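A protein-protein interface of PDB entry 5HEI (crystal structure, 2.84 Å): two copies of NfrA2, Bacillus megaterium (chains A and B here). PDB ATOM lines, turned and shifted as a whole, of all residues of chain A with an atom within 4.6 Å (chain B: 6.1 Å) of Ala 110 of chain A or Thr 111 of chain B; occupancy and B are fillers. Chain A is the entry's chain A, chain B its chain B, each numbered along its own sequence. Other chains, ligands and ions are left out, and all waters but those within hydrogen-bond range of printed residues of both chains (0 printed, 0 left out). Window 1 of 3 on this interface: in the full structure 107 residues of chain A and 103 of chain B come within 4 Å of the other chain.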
ATOM      1  N   ALA A  81       5.314 -17.673 -12.746  1.00  0.00           N
ATOM      2  CA  ALA A  81       4.904 -18.982 -12.246  1.00  0.00           C
ATOM      3  C   ALA A  81       5.577 -19.123 -10.876  1.00  0.00           C
ATOM      4  O   ALA A  81       6.792 -18.952 -10.777  1.00  0.00           O
ATOM      5  CB  ALA A  81       5.369 -20.076 -13.188  1.00  0.00           C
ATOM      6  N   ILE A 106       6.263 -27.023 -14.727  1.00  0.00           N
ATOM      7  CA  ILE A 106       6.435 -26.029 -15.786  1.00  0.00           C
ATOM      8  C   ILE A 106       5.098 -25.839 -16.513  1.00  0.00           C
ATOM      9  O   ILE A 106       4.686 -24.696 -16.722  1.00  0.00           O
ATOM     10  CB  ILE A 106       7.590 -26.404 -16.764  1.00  0.00           C
ATOM     11  CG1 ILE A 106       8.877 -26.895 -16.038  1.00  0.00           C
ATOM     12  CG2 ILE A 106       7.882 -25.289 -17.772  1.00  0.00           C
ATOM     13  CD1 ILE A 106       9.545 -25.935 -15.050  1.00  0.00           C
ATOM     14  N   LEU A 107       4.411 -26.951 -16.868  1.00  0.00           N
ATOM     15  CA  LEU A 107       3.115 -26.898 -17.551  1.00  0.00           C
ATOM     16  C   LEU A 107       2.015 -26.283 -16.691  1.00  0.00           C
ATOM     17  O   LEU A 107       1.208 -25.521 -17.216  1.00  0.00           O
ATOM     18  CB  LEU A 107       2.690 -28.267 -18.104  1.00  0.00           C
ATOM     19  CG  LEU A 107       3.407 -28.775 -19.363  1.00  0.00           C
ATOM     20  CD1 LEU A 107       2.738 -30.022 -19.887  1.00  0.00           C
ATOM     21  CD2 LEU A 107       3.369 -27.749 -20.479  1.00  0.00           C
ATOM     22  N   VAL A 108       2.008 -26.592 -15.372  1.00  0.00           N
ATOM     23  CA  VAL A 108       1.056 -26.061 -14.380  1.00  0.00           C
ATOM     24  C   VAL A 108       1.241 -24.538 -14.214  1.00  0.00           C
ATOM     25  O   VAL A 108       0.257 -23.803 -14.284  1.00  0.00           O
ATOM     26  CB  VAL A 108       1.107 -26.830 -13.020  1.00  0.00           C
ATOM     27  CG1 VAL A 108       0.376 -26.080 -11.908  1.00  0.00           C
ATOM     28  CG2 VAL A 108       0.554 -28.242 -13.158  1.00  0.00           C
ATOM     29  N   GLY A 109       2.494 -24.103 -14.018  1.00  0.00           N
ATOM     30  CA  GLY A 109       2.886 -22.709 -13.840  1.00  0.00           C
ATOM     31  C   GLY A 109       2.603 -21.801 -15.024  1.00  0.00           C
ATOM     32  O   GLY A 109       2.144 -20.672 -14.833  1.00  0.00           O
ATOM     33  N   ALA A 110       2.879 -22.289 -16.257  1.00  0.00           N
ATOM     34  CA  ALA A 110       2.660 -21.553 -17.510  1.00  0.00           C
ATOM     35  C   ALA A 110       1.174 -21.469 -17.881  1.00  0.00           C
ATOM     36  O   ALA A 110       0.720 -20.412 -18.331  1.00  0.00           O
ATOM     37  CB  ALA A 110       3.445 -22.189 -18.640  1.00  0.00           C
ATOM     38  N   THR A 111       0.418 -22.578 -17.700  1.00  0.00           N
ATOM     39  CA  THR A 111      -1.016 -22.606 -17.987  1.00  0.00           C
ATOM     40  C   THR A 111      -1.781 -21.694 -17.028  1.00  0.00           C
ATOM     41  O   THR A 111      -2.641 -20.944 -17.481  1.00  0.00           O
ATOM     42  CB  THR A 111      -1.555 -24.045 -18.176  1.00  0.00           C
ATOM     43  OG1 THR A 111      -2.597 -24.029 -19.148  1.00  0.00           O
ATOM     44  CG2 THR A 111      -2.055 -24.693 -16.893  1.00  0.00           C
ATOM     45  N   ASP A 112      -1.416 -21.719 -15.721  1.00  0.00           N
ATOM     46  CA  ASP A 112      -2.018 -20.899 -14.664  1.00  0.00           C
ATOM     47  C   ASP A 112      -1.775 -19.404 -14.897  1.00  0.00           C
ATOM     48  O   ASP A 112      -2.672 -18.602 -14.639  1.00  0.00           O
ATOM     49  CB  ASP A 112      -1.510 -21.320 -13.271  1.00  0.00           C
ATOM     50  CG  ASP A 112      -2.302 -22.424 -12.580  1.00  0.00           C
ATOM     51  OD1 ASP A 112      -2.612 -23.445 -13.244  1.00  0.00           O
ATOM     52  OD2 ASP A 112      -2.543 -22.304 -11.359  1.00  0.00           O
ATOM     53  N   ALA A 113      -0.571 -19.033 -15.391  1.00  0.00           N
ATOM     54  CA  ALA A 113      -0.197 -17.649 -15.696  1.00  0.00           C
ATOM     55  C   ALA A 113      -0.979 -17.093 -16.899  1.00  0.00           C
ATOM     56  O   ALA A 113      -1.248 -15.893 -16.940  1.00  0.00           O
ATOM     57  CB  ALA A 113       1.299 -17.542 -15.933  1.00  0.00           C
ATOM     58  N   GLY A 114      -1.342 -17.969 -17.840  1.00  0.00           N
ATOM     59  CA  GLY A 114      -2.149 -17.636 -19.010  1.00  0.00           C
ATOM     60  C   GLY A 114      -3.589 -17.365 -18.616  1.00  0.00           C
ATOM     61  O   GLY A 114      -4.231 -16.464 -19.164  1.00  0.00           O
ATOM     62  N   VAL A 157       6.763 -15.591 -16.770  1.00  0.00           N
ATOM     63  CA  VAL A 157       6.012 -16.191 -17.875  1.00  0.00           C
ATOM     64  C   VAL A 157       5.736 -15.151 -18.956  1.00  0.00           C
ATOM     65  O   VAL A 157       6.229 -15.292 -20.074  1.00  0.00           O
ATOM     66  CB  VAL A 157       4.727 -16.927 -17.405  1.00  0.00           C
ATOM     67  CG1 VAL A 157       4.023 -17.612 -18.575  1.00  0.00           C
ATOM     68  CG2 VAL A 157       5.041 -17.939 -16.303  1.00  0.00           C
ATOM     69  N   ILE B 106       7.023 -24.923 -25.744  1.00  0.00           N
ATOM     70  CA  ILE B 106       6.250 -25.513 -24.648  1.00  0.00           C
ATOM     71  C   ILE B 106       5.622 -24.383 -23.817  1.00  0.00           C
ATOM     72  O   ILE B 106       4.427 -24.440 -23.527  1.00  0.00           O
ATOM     73  CB  ILE B 106       7.106 -26.481 -23.776  1.00  0.00           C
ATOM     74  CG1 ILE B 106       8.000 -27.446 -24.608  1.00  0.00           C
ATOM     75  CG2 ILE B 106       6.262 -27.222 -22.735  1.00  0.00           C
ATOM     76  CD1 ILE B 106       7.305 -28.378 -25.586  1.00  0.00           C
ATOM     77  N   LEU B 107       6.415 -23.344 -23.473  1.00  0.00           N
ATOM     78  CA  LEU B 107       5.927 -22.199 -22.700  1.00  0.00           C
ATOM     79  C   LEU B 107       4.877 -21.376 -23.443  1.00  0.00           C
ATOM     80  O   LEU B 107       3.913 -20.940 -22.818  1.00  0.00           O
ATOM     81  CB  LEU B 107       7.075 -21.310 -22.189  1.00  0.00           C
ATOM     82  CG  LEU B 107       7.919 -21.844 -21.017  1.00  0.00           C
ATOM     83  CD1 LEU B 107       8.872 -20.781 -20.521  1.00  0.00           C
ATOM     84  CD2 LEU B 107       7.042 -22.276 -19.842  1.00  0.00           C
ATOM     85  N   VAL B 108       5.045 -21.196 -24.775  1.00  0.00           N
ATOM     86  CA  VAL B 108       4.104 -20.466 -25.643  1.00  0.00           C
ATOM     87  C   VAL B 108       2.767 -21.225 -25.696  1.00  0.00           C
ATOM     88  O   VAL B 108       1.721 -20.645 -25.399  1.00  0.00           O
ATOM     89  CB  VAL B 108       4.687 -20.195 -27.066  1.00  0.00           C
ATOM     90  CG1 VAL B 108       3.613 -19.718 -28.040  1.00  0.00           C
ATOM     91  CG2 VAL B 108       5.834 -19.191 -27.012  1.00  0.00           C
ATOM     92  N   GLY B 109       2.842 -22.513 -26.036  1.00  0.00           N
ATOM     93  CA  GLY B 109       1.702 -23.413 -26.159  1.00  0.00           C
ATOM     94  C   GLY B 109       0.848 -23.551 -24.916  1.00  0.00           C
ATOM     95  O   GLY B 109      -0.380 -23.540 -25.020  1.00  0.00           O
ATOM     96  N   ALA B 110       1.491 -23.676 -23.735  1.00  0.00           N
ATOM     97  CA  ALA B 110       0.819 -23.808 -22.435  1.00  0.00           C
ATOM     98  C   ALA B 110       0.198 -22.489 -21.955  1.00  0.00           C
ATOM     99  O   ALA B 110      -0.916 -22.512 -21.426  1.00  0.00           O
ATOM    100  CB  ALA B 110       1.786 -24.345 -21.390  1.00  0.00           C
ATOM    101  N   THR B 111       0.909 -21.352 -22.138  1.00  0.00           N
ATOM    102  CA  THR B 111       0.417 -20.029 -21.743  1.00  0.00           C
ATOM    103  C   THR B 111      -0.790 -19.636 -22.601  1.00  0.00           C
ATOM    104  O   THR B 111      -1.801 -19.203 -22.049  1.00  0.00           O
ATOM    105  CB  THR B 111       1.543 -18.977 -21.757  1.00  0.00           C
ATOM    106  OG1 THR B 111       2.669 -19.467 -21.028  1.00  0.00           O
ATOM    107  CG2 THR B 111       1.114 -17.641 -21.184  1.00  0.00           C
ATOM    108  N   ASP B 112      -0.695 -19.815 -23.939  1.00  0.00           N
ATOM    109  CA  ASP B 112      -1.771 -19.501 -24.890  1.00  0.00           C
ATOM    110  C   ASP B 112      -3.023 -20.361 -24.666  1.00  0.00           C
ATOM    111  O   ASP B 112      -4.137 -19.861 -24.840  1.00  0.00           O
ATOM    112  CB  ASP B 112      -1.279 -19.594 -26.352  1.00  0.00           C
ATOM    113  CG  ASP B 112      -0.483 -18.393 -26.873  1.00  0.00           C
ATOM    114  OD1 ASP B 112       0.195 -17.717 -26.057  1.00  0.00           O
ATOM    115  OD2 ASP B 112      -0.493 -18.162 -28.102  1.00  0.00           O
ATOM    116  N   ALA B 113      -2.837 -21.650 -24.274  1.00  0.00           N
ATOM    117  CA  ALA B 113      -3.926 -22.597 -23.981  1.00  0.00           C
ATOM    118  C   ALA B 113      -4.681 -22.193 -22.713  1.00  0.00           C
ATOM    119  O   ALA B 113      -5.907 -22.321 -22.668  1.00  0.00           O
ATOM    120  CB  ALA B 113      -3.384 -24.009 -23.848  1.00  0.00           C
ATOM    121  N   GLY B 114      -3.939 -21.683 -21.720  1.00  0.00           N
ATOM    122  CA  GLY B 114      -4.474 -21.169 -20.462  1.00  0.00           C
ATOM    123  C   GLY B 114      -5.326 -19.932 -20.684  1.00  0.00           C
ATOM    124  O   GLY B 114      -6.364 -19.777 -20.032  1.00  0.00           O
ATOM    125  N   ILE B 115      -4.902 -19.060 -21.642  1.00  0.00           N
ATOM    126  CA  ILE B 115      -5.605 -17.840 -22.069  1.00  0.00           C
ATOM    127  C   ILE B 115      -6.970 -18.231 -22.691  1.00  0.00           C
ATOM    128  O   ILE B 115      -8.009 -17.743 -22.238  1.00  0.00           O
ATOM    129  CB  ILE B 115      -4.711 -16.991 -23.041  1.00  0.00           C
ATOM    130  CG1 ILE B 115      -3.601 -16.247 -22.278  1.00  0.00           C
ATOM    131  CG2 ILE B 115      -5.532 -16.004 -23.865  1.00  0.00           C
ATOM    132  CD1 ILE B 115      -2.333 -16.042 -23.030  1.00  0.00           C
ATOM    133  N   SER B 116      -6.947 -19.142 -23.695  1.00  0.00           N
ATOM    134  CA  SER B 116      -8.112 -19.660 -24.426  1.00  0.00           C
ATOM    135  C   SER B 116      -9.111 -20.414 -23.517  1.00  0.00           C
ATOM    136  O   SER B 116     -10.316 -20.383 -23.784  1.00  0.00           O
ATOM    137  CB  SER B 116      -7.657 -20.547 -25.581  1.00  0.00           C
ATOM    138  OG  SER B 116      -8.503 -20.413 -26.711  1.00  0.00           O
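The side-chain hydroxyl of Thr 111 of chain B lies close to the backbone carbonyl oxygen of Ala 110 of chain A (3.5 Å). The backbone carbonyl oxygen of Ala 110 of chain B is in hydrogen-bond range of the side-chain hydroxyl of Thr 111 of chain A (3.2 Å).
O of Leu 107 of chain B sits at hydrogen-bond distance from OG1 of Thr 111 of chain B (2.6 Å).
Among the printed residues, pairs that only touch across the chains: Gly 114 of chain A with Ile 115 of chain B, Val 157 of chain A with Thr 111 of chain B, Gly 114 of chain A with Thr 111 of chain B, Thr 111 of chain A with Gly 114 of chain B, Leu 107 of chain A with Ile 106 of chain B, Gly 114 of chain A with Gly 114 of chain B, Ile 106 of chain A with Leu 107 of chain B, Ala 110 of chain A with Leu 107 of chain B, Leu 107 of chain A with Ala 110 of chain B and Ala 110 of chain A with Ala 110 of chain B.
Of the printed residues of chain B, Leu 107 of chain A touches Ile 106 and Ala 110. Of chain B, only Leu 107 (3.8 Å), Ala 110 (3.9 Å) and Thr 111 (3.4 Å) come within 4 Å of Ala 110 of chain A. Of the printed residues of chain B, Val 157 of chain A touches Thr 111 (3.4 Å). Printed residues of chain A within 4 Å of Ile 106 of chain B: Leu 107 (3.7 Å). The nearest printed residue of chain A that does not touch Thr 111 of chain B is Thr 111 of chain A (4.6 Å). The nearest printed residue of chain B that does not touch Val 157 of chain A is Leu 107 of chain B (5.4 Å).
Hydrophobic or aromatic side chains of chain B within 4 Å of the printed part of chain A: Ile 106, Leu 107, Ala 110 and Ile 115. Printed residues of chain A that touch a printed residue of chain B: Ile 106, Leu 107, Ala 110, Thr 111, Gly 114 and Val 157. Hydrophobic or aromatic side chains of chain A within 4 Å of the printed part of chain B: Ile 106, Leu 107, Ala 110 and Val 157. Among the printed residues, 12 pairs touch across the chains. Among the printed residues, no Asp or Glu carboxylate lies within 4 Å of a Lys or Arg side-chain nitrogen of the other chain.
Ile 106 of chain A touches Leu 107 of chain B, and with the chains exchanged Leu 107 of chain A touches Ile 106 of chain B. Ala 110 of chain A touches Thr 111 of chain B, and with the chains exchanged Thr 111 of chain A touches Ala 110 of chain B. Thr 111 of chain A touches Gly 114 of chain B, and with the chains exchanged Gly 114 of chain A touches Thr 111 of chain B. Gly 114 of chain A touches its own counterpart, Gly 114 of chain B. Positions printed for both chains: 106, 107, 108, 109, 110, 111, 112, 113 and 114.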
